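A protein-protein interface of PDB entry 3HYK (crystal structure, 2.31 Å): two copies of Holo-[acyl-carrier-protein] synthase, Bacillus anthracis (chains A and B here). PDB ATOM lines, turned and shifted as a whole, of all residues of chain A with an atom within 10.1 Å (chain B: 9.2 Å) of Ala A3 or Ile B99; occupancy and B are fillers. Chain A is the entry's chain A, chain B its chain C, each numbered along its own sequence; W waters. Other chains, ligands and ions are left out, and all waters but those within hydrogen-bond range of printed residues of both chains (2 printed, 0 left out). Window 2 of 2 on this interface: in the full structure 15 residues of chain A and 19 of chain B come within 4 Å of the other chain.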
ATOM      1  N   ASN A   2     -12.083 -11.080   4.902  1.00  0.00           N
ATOM      2  CA  ASN A   2     -12.576 -12.147   3.989  1.00  0.00           C
ATOM      3  C   ASN A   2     -12.995 -11.547   2.642  1.00  0.00           C
ATOM      4  O   ASN A   2     -14.165 -11.248   2.415  1.00  0.00           O
ATOM      5  CB  ASN A   2     -13.733 -12.886   4.651  1.00  0.00           C
ATOM      6  CG  ASN A   2     -13.399 -13.321   6.065  1.00  0.00           C
ATOM      7  OD1 ASN A   2     -12.383 -12.901   6.625  1.00  0.00           O
ATOM      8  ND2 ASN A   2     -14.256 -14.147   6.662  1.00  0.00           N
ATOM      9  N   ALA A   3     -12.014 -11.385   1.754  1.00  0.00           N
ATOM     10  CA  ALA A   3     -12.217 -10.781   0.428  1.00  0.00           C
ATOM     11  C   ALA A   3     -13.496 -11.212  -0.291  1.00  0.00           C
ATOM     12  O   ALA A   3     -13.866 -12.387  -0.295  1.00  0.00           O
ATOM     13  CB  ALA A   3     -10.985 -11.038  -0.485  1.00  0.00           C
ATOM     14  N   MET A   4     -14.164 -10.232  -0.894  1.00  0.00           N
ATOM     15  CA  MET A   4     -15.357 -10.478  -1.672  1.00  0.00           C
ATOM     16  C   MET A   4     -14.963 -10.942  -3.058  1.00  0.00           C
ATOM     17  O   MET A   4     -15.741 -11.608  -3.712  1.00  0.00           O
ATOM     18  CB  MET A   4     -16.240  -9.236  -1.741  1.00  0.00           C
ATOM     19  CG  MET A   4     -16.830  -8.834  -0.379  1.00  0.00           C
ATOM     20  SD  MET A   4     -17.974 -10.234   0.452  1.00  0.00           S
ATOM     21  CE  MET A   4     -19.499 -10.278  -0.800  1.00  0.00           C
ATOM     22  N   ILE A   5     -13.763 -10.585  -3.504  1.00  0.00           N
ATOM     23  CA  ILE A   5     -13.258 -11.053  -4.792  1.00  0.00           C
ATOM     24  C   ILE A   5     -12.327 -12.228  -4.510  1.00  0.00           C
ATOM     25  O   ILE A   5     -11.342 -12.074  -3.794  1.00  0.00           O
ATOM     26  CB  ILE A   5     -12.538  -9.930  -5.571  1.00  0.00           C
ATOM     27  CG1 ILE A   5     -13.568  -8.875  -5.981  1.00  0.00           C
ATOM     28  CG2 ILE A   5     -11.872 -10.475  -6.815  1.00  0.00           C
ATOM     29  CD1 ILE A   5     -13.019  -7.690  -6.691  1.00  0.00           C
ATOM     30  N   VAL A   6     -12.651 -13.407  -5.034  1.00  0.00           N
ATOM     31  CA  VAL A   6     -11.809 -14.583  -4.782  1.00  0.00           C
ATOM     32  C   VAL A   6     -10.591 -14.546  -5.706  1.00  0.00           C
ATOM     33  O   VAL A   6      -9.511 -14.993  -5.331  1.00  0.00           O
ATOM     34  CB  VAL A   6     -12.564 -15.924  -4.940  1.00  0.00           C
ATOM     35  CG1 VAL A   6     -13.912 -15.849  -4.270  1.00  0.00           C
ATOM     36  CG2 VAL A   6     -12.769 -16.250  -6.366  1.00  0.00           C
ATOM     37  N   GLY A   7     -10.750 -13.983  -6.905  1.00  0.00           N
ATOM     38  CA  GLY A   7      -9.632 -13.884  -7.833  1.00  0.00           C
ATOM     39  C   GLY A   7     -10.025 -13.228  -9.129  1.00  0.00           C
ATOM     40  O   GLY A   7     -11.216 -13.102  -9.425  1.00  0.00           O
ATOM     41  N   ILE A   8      -9.016 -12.813  -9.903  1.00  0.00           N
ATOM     42  CA  ILE A   8      -9.250 -12.205 -11.217  1.00  0.00           C
ATOM     43  C   ILE A   8      -8.329 -12.872 -12.240  1.00  0.00           C
ATOM     44  O   ILE A   8      -7.277 -13.400 -11.885  1.00  0.00           O
ATOM     45  CB  ILE A   8      -9.041 -10.635 -11.198  1.00  0.00           C
ATOM     46  CG1 ILE A   8      -7.559 -10.242 -11.254  1.00  0.00           C
ATOM     47  CG2 ILE A   8      -9.699 -10.028  -9.958  1.00  0.00           C
ATOM     48  CD1 ILE A   8      -7.322  -8.691 -11.229  1.00  0.00           C
ATOM     49  N   HIS A  98     -18.994 -19.684  -6.630  1.00  0.00           N
ATOM     50  CA  HIS A  98     -18.793 -18.258  -6.756  1.00  0.00           C
ATOM     51  C   HIS A  98     -19.589 -17.617  -7.892  1.00  0.00           C
ATOM     52  O   HIS A  98     -20.136 -18.304  -8.737  1.00  0.00           O
ATOM     53  CB  HIS A  98     -17.311 -17.968  -6.949  1.00  0.00           C
ATOM     54  CG  HIS A  98     -16.445 -18.566  -5.895  1.00  0.00           C
ATOM     55  ND1 HIS A  98     -16.690 -18.395  -4.549  1.00  0.00           N
ATOM     56  CD2 HIS A  98     -15.299 -19.285  -5.983  1.00  0.00           C
ATOM     57  CE1 HIS A  98     -15.758 -19.022  -3.853  1.00  0.00           C
ATOM     58  NE2 HIS A  98     -14.895 -19.558  -4.699  1.00  0.00           N
ATOM     59  N   VAL A 116     -13.730 -11.903 -13.237  1.00  0.00           N
ATOM     60  CA  VAL A 116     -13.668 -11.523 -11.837  1.00  0.00           C
ATOM     61  C   VAL A 116     -14.592 -12.497 -11.151  1.00  0.00           C
ATOM     62  O   VAL A 116     -15.758 -12.614 -11.518  1.00  0.00           O
ATOM     63  CB  VAL A 116     -14.119 -10.070 -11.575  1.00  0.00           C
ATOM     64  CG1 VAL A 116     -14.237  -9.795 -10.069  1.00  0.00           C
ATOM     65  CG2 VAL A 116     -13.144  -9.092 -12.232  1.00  0.00           C
ATOM     66  N   LEU A 117     -14.050 -13.243 -10.201  1.00  0.00           N
ATOM     67  CA  LEU A 117     -14.835 -14.193  -9.406  1.00  0.00           C
ATOM     68  C   LEU A 117     -15.131 -13.512  -8.104  1.00  0.00           C
ATOM     69  O   LEU A 117     -14.225 -13.014  -7.435  1.00  0.00           O
ATOM     70  CB  LEU A 117     -14.068 -15.493  -9.117  1.00  0.00           C
ATOM     71  CG  LEU A 117     -13.781 -16.474 -10.261  1.00  0.00           C
ATOM     72  CD1 LEU A 117     -13.027 -17.722  -9.730  1.00  0.00           C
ATOM     73  CD2 LEU A 117     -15.110 -16.867 -10.936  1.00  0.00           C
ATOM     74  N   GLU A 118     -16.408 -13.489  -7.744  1.00  0.00           N
ATOM     75  CA  GLU A 118     -16.855 -12.851  -6.530  1.00  0.00           C
ATOM     76  C   GLU A 118     -17.471 -13.875  -5.578  1.00  0.00           C
ATOM     77  O   GLU A 118     -18.151 -14.802  -6.003  1.00  0.00           O
ATOM     78  CB  GLU A 118     -17.882 -11.768  -6.897  1.00  0.00           C
ATOM     79  CG  GLU A 118     -18.580 -11.100  -5.713  1.00  0.00           C
ATOM     80  CD  GLU A 118     -19.696 -10.135  -6.138  1.00  0.00           C
ATOM     81  OE1 GLU A 118     -19.827  -9.864  -7.342  1.00  0.00           O
ATOM     82  OE2 GLU A 118     -20.456  -9.666  -5.257  1.00  0.00           O
ATOM     83  N   SER A 119     -17.226 -13.698  -4.288  1.00  0.00           N
ATOM     84  CA  SER A 119     -17.781 -14.583  -3.278  1.00  0.00           C
ATOM     85  C   SER A 119     -19.270 -14.390  -3.120  1.00  0.00           C
ATOM     86  O   SER A 119     -19.764 -13.273  -3.104  1.00  0.00           O
ATOM     87  CB  SER A 119     -17.134 -14.331  -1.919  1.00  0.00           C
ATOM     88  OG  SER A 119     -15.761 -14.681  -1.947  1.00  0.00           O
ATOM     89  N   SER A 120     -19.978 -15.502  -2.999  1.00  0.00           N
ATOM     90  CA  SER A 120     -21.416 -15.496  -2.768  1.00  0.00           C
ATOM     91  C   SER A 120     -21.551 -15.782  -1.292  1.00  0.00           C
ATOM     92  O   SER A 120     -22.295 -16.672  -0.893  1.00  0.00           O
ATOM     93  CB  SER A 120     -22.071 -16.616  -3.551  1.00  0.00           C
ATOM     94  OG  SER A 120     -21.568 -17.857  -3.086  1.00  0.00           O
ATOM     95  N   SER A 121     -20.789 -15.027  -0.504  1.00  0.00           N
ATOM     96  CA  SER A 121     -20.688 -15.163   0.950  1.00  0.00           C
ATOM     97  C   SER A 121     -19.263 -14.756   1.319  1.00  0.00           C
ATOM     98  O   SER A 121     -18.992 -14.357   2.447  1.00  0.00           O
ATOM     99  CB  SER A 121     -20.942 -16.598   1.443  1.00  0.00           C
ATOM    100  OG  SER A 121     -22.312 -16.971   1.396  1.00  0.00           O
ATOM    101  N   MET B   4     -16.350  -1.186  -1.672  1.00  0.00           N
ATOM    102  CA  MET B   4     -15.545  -2.394  -1.884  1.00  0.00           C
ATOM    103  C   MET B   4     -14.270  -2.162  -2.706  1.00  0.00           C
ATOM    104  O   MET B   4     -13.174  -2.250  -2.165  1.00  0.00           O
ATOM    105  CB  MET B   4     -16.420  -3.508  -2.507  1.00  0.00           C
ATOM    106  CG  MET B   4     -15.682  -4.795  -2.933  1.00  0.00           C
ATOM    107  SD  MET B   4     -16.862  -6.232  -3.623  1.00  0.00           S
ATOM    108  CE  MET B   4     -17.881  -5.235  -4.954  1.00  0.00           C
ATOM    109  N   ILE B   5     -14.402  -1.864  -3.995  1.00  0.00           N
ATOM    110  CA  ILE B   5     -13.226  -1.663  -4.855  1.00  0.00           C
ATOM    111  C   ILE B   5     -12.619  -0.273  -4.622  1.00  0.00           C
ATOM    112  O   ILE B   5     -13.344   0.714  -4.646  1.00  0.00           O
ATOM    113  CB  ILE B   5     -13.606  -1.758  -6.362  1.00  0.00           C
ATOM    114  CG1 ILE B   5     -14.372  -3.041  -6.697  1.00  0.00           C
ATOM    115  CG2 ILE B   5     -12.385  -1.588  -7.245  1.00  0.00           C
ATOM    116  CD1 ILE B   5     -13.627  -4.280  -6.511  1.00  0.00           C
ATOM    117  N   VAL B   6     -11.311  -0.178  -4.388  1.00  0.00           N
ATOM    118  CA  VAL B   6     -10.679   1.140  -4.222  1.00  0.00           C
ATOM    119  C   VAL B   6     -10.231   1.650  -5.594  1.00  0.00           C
ATOM    120  O   VAL B   6     -10.120   2.853  -5.801  1.00  0.00           O
ATOM    121  CB  VAL B   6      -9.450   1.167  -3.251  1.00  0.00           C
ATOM    122  CG1 VAL B   6      -9.791   0.559  -1.903  1.00  0.00           C
ATOM    123  CG2 VAL B   6      -8.319   0.447  -3.821  1.00  0.00           C
ATOM    124  N   GLY B   7      -9.973   0.742  -6.537  1.00  0.00           N
ATOM    125  CA  GLY B   7      -9.556   1.151  -7.873  1.00  0.00           C
ATOM    126  C   GLY B   7      -9.180  -0.047  -8.711  1.00  0.00           C
ATOM    127  O   GLY B   7      -8.946  -1.132  -8.172  1.00  0.00           O
ATOM    128  N   TYR B  63      -0.968  -1.609 -11.297  1.00  0.00           N
ATOM    129  CA  TYR B  63      -1.196  -1.409  -9.869  1.00  0.00           C
ATOM    130  C   TYR B  63      -1.229   0.095  -9.552  1.00  0.00           C
ATOM    131  O   TYR B  63      -2.150   0.593  -8.890  1.00  0.00           O
ATOM    132  CB  TYR B  63      -0.102  -2.105  -9.041  1.00  0.00           C
ATOM    133  CG  TYR B  63      -0.137  -1.692  -7.598  1.00  0.00           C
ATOM    134  CD1 TYR B  63      -1.086  -2.217  -6.733  1.00  0.00           C
ATOM    135  CD2 TYR B  63       0.764  -0.754  -7.099  1.00  0.00           C
ATOM    136  CE1 TYR B  63      -1.140  -1.823  -5.427  1.00  0.00           C
ATOM    137  CE2 TYR B  63       0.695  -0.328  -5.783  1.00  0.00           C
ATOM    138  CZ  TYR B  63      -0.257  -0.879  -4.953  1.00  0.00           C
ATOM    139  OH  TYR B  63      -0.316  -0.521  -3.635  1.00  0.00           O
ATOM    140  N   ALA B  66      -4.382   1.636 -10.506  1.00  0.00           N
ATOM    141  CA  ALA B  66      -5.390   1.227  -9.551  1.00  0.00           C
ATOM    142  C   ALA B  66      -5.331   2.180  -8.365  1.00  0.00           C
ATOM    143  O   ALA B  66      -6.363   2.578  -7.842  1.00  0.00           O
ATOM    144  CB  ALA B  66      -5.157  -0.243  -9.108  1.00  0.00           C
ATOM    145  N   LYS B  89       0.585 -18.613 -10.198  1.00  0.00           N
ATOM    146  CA  LYS B  89      -0.226 -17.412 -10.044  1.00  0.00           C
ATOM    147  C   LYS B  89       0.600 -16.228  -9.516  1.00  0.00           C
ATOM    148  O   LYS B  89       1.260 -16.340  -8.491  1.00  0.00           O
ATOM    149  CB  LYS B  89      -1.399 -17.684  -9.087  1.00  0.00           C
ATOM    150  CG  LYS B  89      -2.312 -16.470  -8.808  1.00  0.00           C
ATOM    151  CD  LYS B  89      -3.396 -16.837  -7.814  1.00  0.00           C
ATOM    152  CE  LYS B  89      -4.109 -15.610  -7.279  1.00  0.00           C
ATOM    153  NZ  LYS B  89      -3.233 -14.773  -6.384  1.00  0.00           N
ATOM    154  N   LEU B  92       1.162  -9.888  -6.136  1.00  0.00           N
ATOM    155  CA  LEU B  92       1.757  -8.576  -6.011  1.00  0.00           C
ATOM    156  C   LEU B  92       1.978  -8.247  -4.532  1.00  0.00           C
ATOM    157  O   LEU B  92       1.034  -8.241  -3.734  1.00  0.00           O
ATOM    158  CB  LEU B  92       0.883  -7.538  -6.690  1.00  0.00           C
ATOM    159  CG  LEU B  92       1.523  -6.150  -6.908  1.00  0.00           C
ATOM    160  CD1 LEU B  92       0.952  -5.478  -8.164  1.00  0.00           C
ATOM    161  CD2 LEU B  92       1.411  -5.243  -5.689  1.00  0.00           C
ATOM    162  N   THR B  94       3.453  -5.389  -2.005  1.00  0.00           N
ATOM    163  CA  THR B  94       3.839  -3.991  -1.833  1.00  0.00           C
ATOM    164  C   THR B  94       3.265  -3.496  -0.515  1.00  0.00           C
ATOM    165  O   THR B  94       2.511  -4.212   0.121  1.00  0.00           O
ATOM    166  CB  THR B  94       3.379  -3.105  -3.025  1.00  0.00           C
ATOM    167  OG1 THR B  94       4.073  -1.856  -2.971  1.00  0.00           O
ATOM    168  CG2 THR B  94       1.896  -2.875  -2.997  1.00  0.00           C
ATOM    169  N   SER B  95       3.669  -2.307  -0.076  1.00  0.00           N
ATOM    170  CA  SER B  95       3.153  -1.730   1.173  1.00  0.00           C
ATOM    171  C   SER B  95       1.771  -1.140   0.945  1.00  0.00           C
ATOM    172  O   SER B  95       1.658  -0.125   0.268  1.00  0.00           O
ATOM    173  CB  SER B  95       4.029  -0.571   1.636  1.00  0.00           C
ATOM    174  OG  SER B  95       5.362  -0.958   1.854  1.00  0.00           O
ATOM    175  N   THR B  96       0.729  -1.741   1.504  1.00  0.00           N
ATOM    176  CA  THR B  96      -0.626  -1.213   1.347  1.00  0.00           C
ATOM    177  C   THR B  96      -1.579  -1.844   2.340  1.00  0.00           C
ATOM    178  O   THR B  96      -1.348  -2.950   2.799  1.00  0.00           O
ATOM    179  CB  THR B  96      -1.205  -1.539  -0.036  1.00  0.00           C
ATOM    180  OG1 THR B  96      -0.371  -0.981  -1.043  1.00  0.00           O
ATOM    181  CG2 THR B  96      -2.561  -0.949  -0.187  1.00  0.00           C
ATOM    182  N   GLU B  97      -2.665  -1.144   2.632  1.00  0.00           N
ATOM    183  CA  GLU B  97      -3.710  -1.653   3.510  1.00  0.00           C
ATOM    184  C   GLU B  97      -4.717  -2.471   2.715  1.00  0.00           C
ATOM    185  O   GLU B  97      -5.585  -3.133   3.279  1.00  0.00           O
ATOM    186  CB  GLU B  97      -4.480  -0.490   4.103  1.00  0.00           C
ATOM    187  CG  GLU B  97      -3.700   0.356   5.057  1.00  0.00           C
ATOM    188  CD  GLU B  97      -4.396   1.668   5.319  1.00  0.00           C
ATOM    189  OE1 GLU B  97      -4.859   2.279   4.326  1.00  0.00           O
ATOM    190  OE2 GLU B  97      -4.450   2.092   6.495  1.00  0.00           O
ATOM    191  N   HIS B  98      -4.603  -2.414   1.402  1.00  0.00           N
ATOM    192  CA  HIS B  98      -5.556  -3.075   0.546  1.00  0.00           C
ATOM    193  C   HIS B  98      -5.151  -4.463   0.062  1.00  0.00           C
ATOM    194  O   HIS B  98      -3.983  -4.857   0.107  1.00  0.00           O
ATOM    195  CB  HIS B  98      -5.838  -2.192  -0.670  1.00  0.00           C
ATOM    196  CG  HIS B  98      -6.230  -0.792  -0.322  1.00  0.00           C
ATOM    197  ND1 HIS B  98      -5.632   0.316  -0.891  1.00  0.00           N
ATOM    198  CD2 HIS B  98      -7.131  -0.318   0.571  1.00  0.00           C
ATOM    199  CE1 HIS B  98      -6.175   1.408  -0.389  1.00  0.00           C
ATOM    200  NE2 HIS B  98      -7.087   1.052   0.499  1.00  0.00           N
ATOM    201  N   ILE B  99      -6.156  -5.198  -0.395  1.00  0.00           N
ATOM    202  CA  ILE B  99      -5.962  -6.509  -0.961  1.00  0.00           C
ATOM    203  C   ILE B  99      -5.712  -6.245  -2.443  1.00  0.00           C
ATOM    204  O   ILE B  99      -6.475  -5.512  -3.085  1.00  0.00           O
ATOM    205  CB  ILE B  99      -7.206  -7.376  -0.752  1.00  0.00           C
ATOM    206  CG1 ILE B  99      -7.523  -7.478   0.749  1.00  0.00           C
ATOM    207  CG2 ILE B  99      -7.012  -8.760  -1.351  1.00  0.00           C
ATOM    208  CD1 ILE B  99      -8.834  -8.169   1.053  1.00  0.00           C
ATOM    209  N   VAL B 100      -4.625  -6.804  -2.970  1.00  0.00           N
ATOM    210  CA  VAL B 100      -4.257  -6.620  -4.364  1.00  0.00           C
ATOM    211  C   VAL B 100      -4.552  -7.857  -5.200  1.00  0.00           C
ATOM    212  O   VAL B 100      -4.008  -8.940  -4.957  1.00  0.00           O
ATOM    213  CB  VAL B 100      -2.747  -6.300  -4.499  1.00  0.00           C
ATOM    214  CG1 VAL B 100      -2.390  -6.006  -5.932  1.00  0.00           C
ATOM    215  CG2 VAL B 100      -2.360  -5.109  -3.596  1.00  0.00           C
ATOM    216  N   HIS B 101      -5.432  -7.693  -6.183  1.00  0.00           N
ATOM    217  CA  HIS B 101      -5.747  -8.766  -7.119  1.00  0.00           C
ATOM    218  C   HIS B 101      -5.038  -8.419  -8.409  1.00  0.00           C
ATOM    219  O   HIS B 101      -5.092  -7.283  -8.868  1.00  0.00           O
ATOM    220  CB  HIS B 101      -7.241  -8.912  -7.330  1.00  0.00           C
ATOM    221  CG  HIS B 101      -7.990  -9.159  -6.063  1.00  0.00           C
ATOM    222  ND1 HIS B 101      -7.987 -10.382  -5.424  1.00  0.00           N
ATOM    223  CD2 HIS B 101      -8.765  -8.339  -5.314  1.00  0.00           C
ATOM    224  CE1 HIS B 101      -8.721 -10.298  -4.329  1.00  0.00           C
ATOM    225  NE2 HIS B 101      -9.202  -9.070  -4.238  1.00  0.00           N
ATOM    226  N   LEU B 102      -4.364  -9.410  -8.978  1.00  0.00           N
ATOM    227  CA  LEU B 102      -3.570  -9.245 -10.194  1.00  0.00           C
ATOM    228  C   LEU B 102      -3.664 -10.404 -11.173  1.00  0.00           C
ATOM    229  O   LEU B 102      -3.846 -11.551 -10.770  1.00  0.00           O
ATOM    230  CB  LEU B 102      -2.098  -9.146  -9.783  1.00  0.00           C
ATOM    231  CG  LEU B 102      -1.032  -9.240 -10.869  1.00  0.00           C
ATOM    232  CD1 LEU B 102      -1.057  -8.027 -11.798  1.00  0.00           C
ATOM    233  CD2 LEU B 102       0.319  -9.390 -10.184  1.00  0.00           C
ATOM    234  N   VAL B 115      -5.172  -5.022 -12.472  1.00  0.00           N
ATOM    235  CA  VAL B 115      -5.227  -5.018 -11.029  1.00  0.00           C
ATOM    236  C   VAL B 115      -6.575  -4.483 -10.555  1.00  0.00           C
ATOM    237  O   VAL B 115      -7.168  -3.575 -11.167  1.00  0.00           O
ATOM    238  CB  VAL B 115      -4.068  -4.179 -10.409  1.00  0.00           C
ATOM    239  CG1 VAL B 115      -4.327  -3.886  -8.921  1.00  0.00           C
ATOM    240  CG2 VAL B 115      -2.709  -4.875 -10.622  1.00  0.00           C
ATOM    241  N   VAL B 116      -7.069  -5.119  -9.496  1.00  0.00           N
ATOM    242  CA  VAL B 116      -8.277  -4.698  -8.791  1.00  0.00           C
ATOM    243  C   VAL B 116      -7.810  -4.597  -7.358  1.00  0.00           C
ATOM    244  O   VAL B 116      -7.212  -5.546  -6.828  1.00  0.00           O
ATOM    245  CB  VAL B 116      -9.434  -5.687  -8.893  1.00  0.00           C
ATOM    246  CG1 VAL B 116     -10.635  -5.217  -8.049  1.00  0.00           C
ATOM    247  CG2 VAL B 116      -9.839  -5.857 -10.366  1.00  0.00           C
ATOM    248  N   LEU B 117      -7.988  -3.422  -6.770  1.00  0.00           N
ATOM    249  CA  LEU B 117      -7.642  -3.201  -5.372  1.00  0.00           C
ATOM    250  C   LEU B 117      -8.945  -3.233  -4.591  1.00  0.00           C
ATOM    251  O   LEU B 117      -9.913  -2.538  -4.930  1.00  0.00           O
ATOM    252  CB  LEU B 117      -6.956  -1.857  -5.143  1.00  0.00           C
ATOM    253  CG  LEU B 117      -5.513  -1.593  -5.592  1.00  0.00           C
ATOM    254  CD1 LEU B 117      -5.119  -0.179  -5.137  1.00  0.00           C
ATOM    255  CD2 LEU B 117      -4.513  -2.641  -5.039  1.00  0.00           C
ATOM    256  N   GLU B 118      -8.970  -4.043  -3.542  1.00  0.00           N
ATOM    257  CA  GLU B 118     -10.157  -4.195  -2.722  1.00  0.00           C
ATOM    258  C   GLU B 118      -9.827  -3.740  -1.310  1.00  0.00           C
ATOM    259  O   GLU B 118      -8.710  -3.955  -0.814  1.00  0.00           O
ATOM    260  CB  GLU B 118     -10.591  -5.664  -2.749  1.00  0.00           C
ATOM    261  CG  GLU B 118     -11.730  -6.035  -1.820  1.00  0.00           C
ATOM    262  CD  GLU B 118     -12.036  -7.525  -1.872  1.00  0.00           C
ATOM    263  OE1 GLU B 118     -11.270  -8.284  -2.505  1.00  0.00           O
ATOM    264  OE2 GLU B 118     -13.044  -7.937  -1.282  1.00  0.00           O
ATOM    265  N   SER B 119     -10.799  -3.099  -0.664  1.00  0.00           N
ATOM    266  CA  SER B 119     -10.603  -2.605   0.693  1.00  0.00           C
ATOM    267  C   SER B 119     -10.774  -3.725   1.699  1.00  0.00           C
ATOM    268  O   SER B 119     -11.652  -4.558   1.560  1.00  0.00           O
ATOM    269  CB  SER B 119     -11.634  -1.541   1.022  1.00  0.00           C
ATOM    270  OG  SER B 119     -12.902  -2.154   1.187  1.00  0.00           O
ATOM    271  N   SER B 120      -9.925  -3.740   2.716  1.00  0.00           N
ATOM    272  CA  SER B 120     -10.032  -4.734   3.778  1.00  0.00           C
ATOM    273  C   SER B 120     -10.848  -4.082   4.884  1.00  0.00           C
ATOM    274  O   SER B 120     -10.296  -3.499   5.819  1.00  0.00           O
ATOM    275  CB  SER B 120      -8.655  -5.141   4.282  1.00  0.00           C
ATOM    276  OG  SER B 120      -7.943  -4.004   4.716  1.00  0.00           O
ATOM    277  N   SER B 121     -12.168  -4.171   4.738  1.00  0.00           N
ATOM    278  CA  SER B 121     -13.130  -3.559   5.653  1.00  0.00           C
ATOM    279  C   SER B 121     -14.150  -2.783   4.808  1.00  0.00           C
ATOM    280  O   SER B 121     -14.237  -1.553   4.875  1.00  0.00           O
ATOM    281  CB  SER B 121     -12.449  -2.625   6.671  1.00  0.00           C
ATOM    282  OG  SER B 121     -13.402  -1.974   7.505  1.00  0.00           O
HETATM  283  O   HOH W   1      -4.484 -14.210 -11.414  1.00  0.00           O
HETATM  284  O   HOH W   2      -6.159 -12.871  -8.743  1.00  0.00           O
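The side-chain carboxylate (OE2) of Glu B118 is in hydrogen-bond range of the backbone NH (N) of Met A4.
NE2 of His B101 sits at hydrogen-bond distance from OE1 of Glu B118. O of Val B116 lies within hydrogen-bond range of N of His B101 (2.9 Å). The side-chain hydroxyl of Ser A119 sits at hydrogen-bond distance from the backbone carbonyl oxygen of Ala A3 (3.4 Å). The backbone NH (N) of Ser B119 sits at hydrogen-bond distance from the backbone carbonyl oxygen (O) of Met B4 (2.9 Å). The backbone carbonyl oxygen of Met A4 lies within hydrogen-bond range of the backbone NH of Ser A119 (2.6 Å). O of Glu B118 lies within hydrogen-bond range of N of Ile B99 (2.9 Å).
Ala A3 touches Ile B99. CA of Ala A3 touches OE2 of Glu B118, at 3.4 Å. Met B4 touches Met A4 (SD to CB, 3.6 Å). Ile B5 touches Ile A5 (CD1 to CD1, 3.5 Å). His B101 touches Ile A5. Val B116 touches Ile A5. Ile A5 touches Glu B118 (N to OE2, 3.5 Å). Ile A8 touches His B101. CD1 of Ile A8 touches N of Leu B102 (3.8 Å). Val B116 touches Ile A8 (CG2 to CD1, 3.9 Å).
Of chain B, only Ile B99 (3.9 Å) and Glu B118 (3.4 Å) come within 4 Å of Ala A3. Of chain A, only Ala A3 (3.9 Å) comes within 4 Å of Ile B99. No residue of chain A comes within 4 Å of Val B100. No residue of chain A comes within 4 Å of Leu B117. Of the printed residues of chain A, Glu B118 touches Ala A3, Met A4 and Ile A5. Printed residues of chain A within 4 Å of His B101: Ile A5 and Ile A8. Printed residues of chain A within 4 Å of Val B116: Ile A5 and Ile A8. Of the printed residues of chain A, Ile B5 touches Ile A5. His B98 touches none of the printed residues of chain A. Glu A118 touches none of the printed residues of chain B. The nearest residue of chain B that does not touch Ala A3 is His B101 (4.5 Å). The nearest residue of chain A that does not touch Ile B99 is Asn A2 (5.6 Å).
Of the 14 printed residues of chain A, 4 touch a printed residue of chain B. Hydrophobic or aromatic side chains of chain A that line the printed part of chain B: Ala A3, Met A4, Ile A5 and Ile A8. Of the 24 printed residues of chain B, 7 touch a printed residue of chain A. Hydrophobic or aromatic side chains of chain B that line the printed part of chain A: Met B4, Ile B5, Ile B99, His B101 and Val B116. Among the printed residues, 11 pairs touch across the chains.
Met A4 touches its own counterpart, Met B4. Met A4 touches Glu B118, but with the chains exchanged Glu A118 does not touch Met B4 (5.1 Å). Ile A5 touches its own counterpart, Ile B5. Ile A5 touches Glu B118, but with the chains exchanged Glu A118 does not touch Ile B5 (8.4 Å).
Water W1 bridges O of Leu B102 (2.8 Å) and O of Ile A8 (2.9 Å). Water W2 bridges N of Ile A8 and O of Leu B102.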
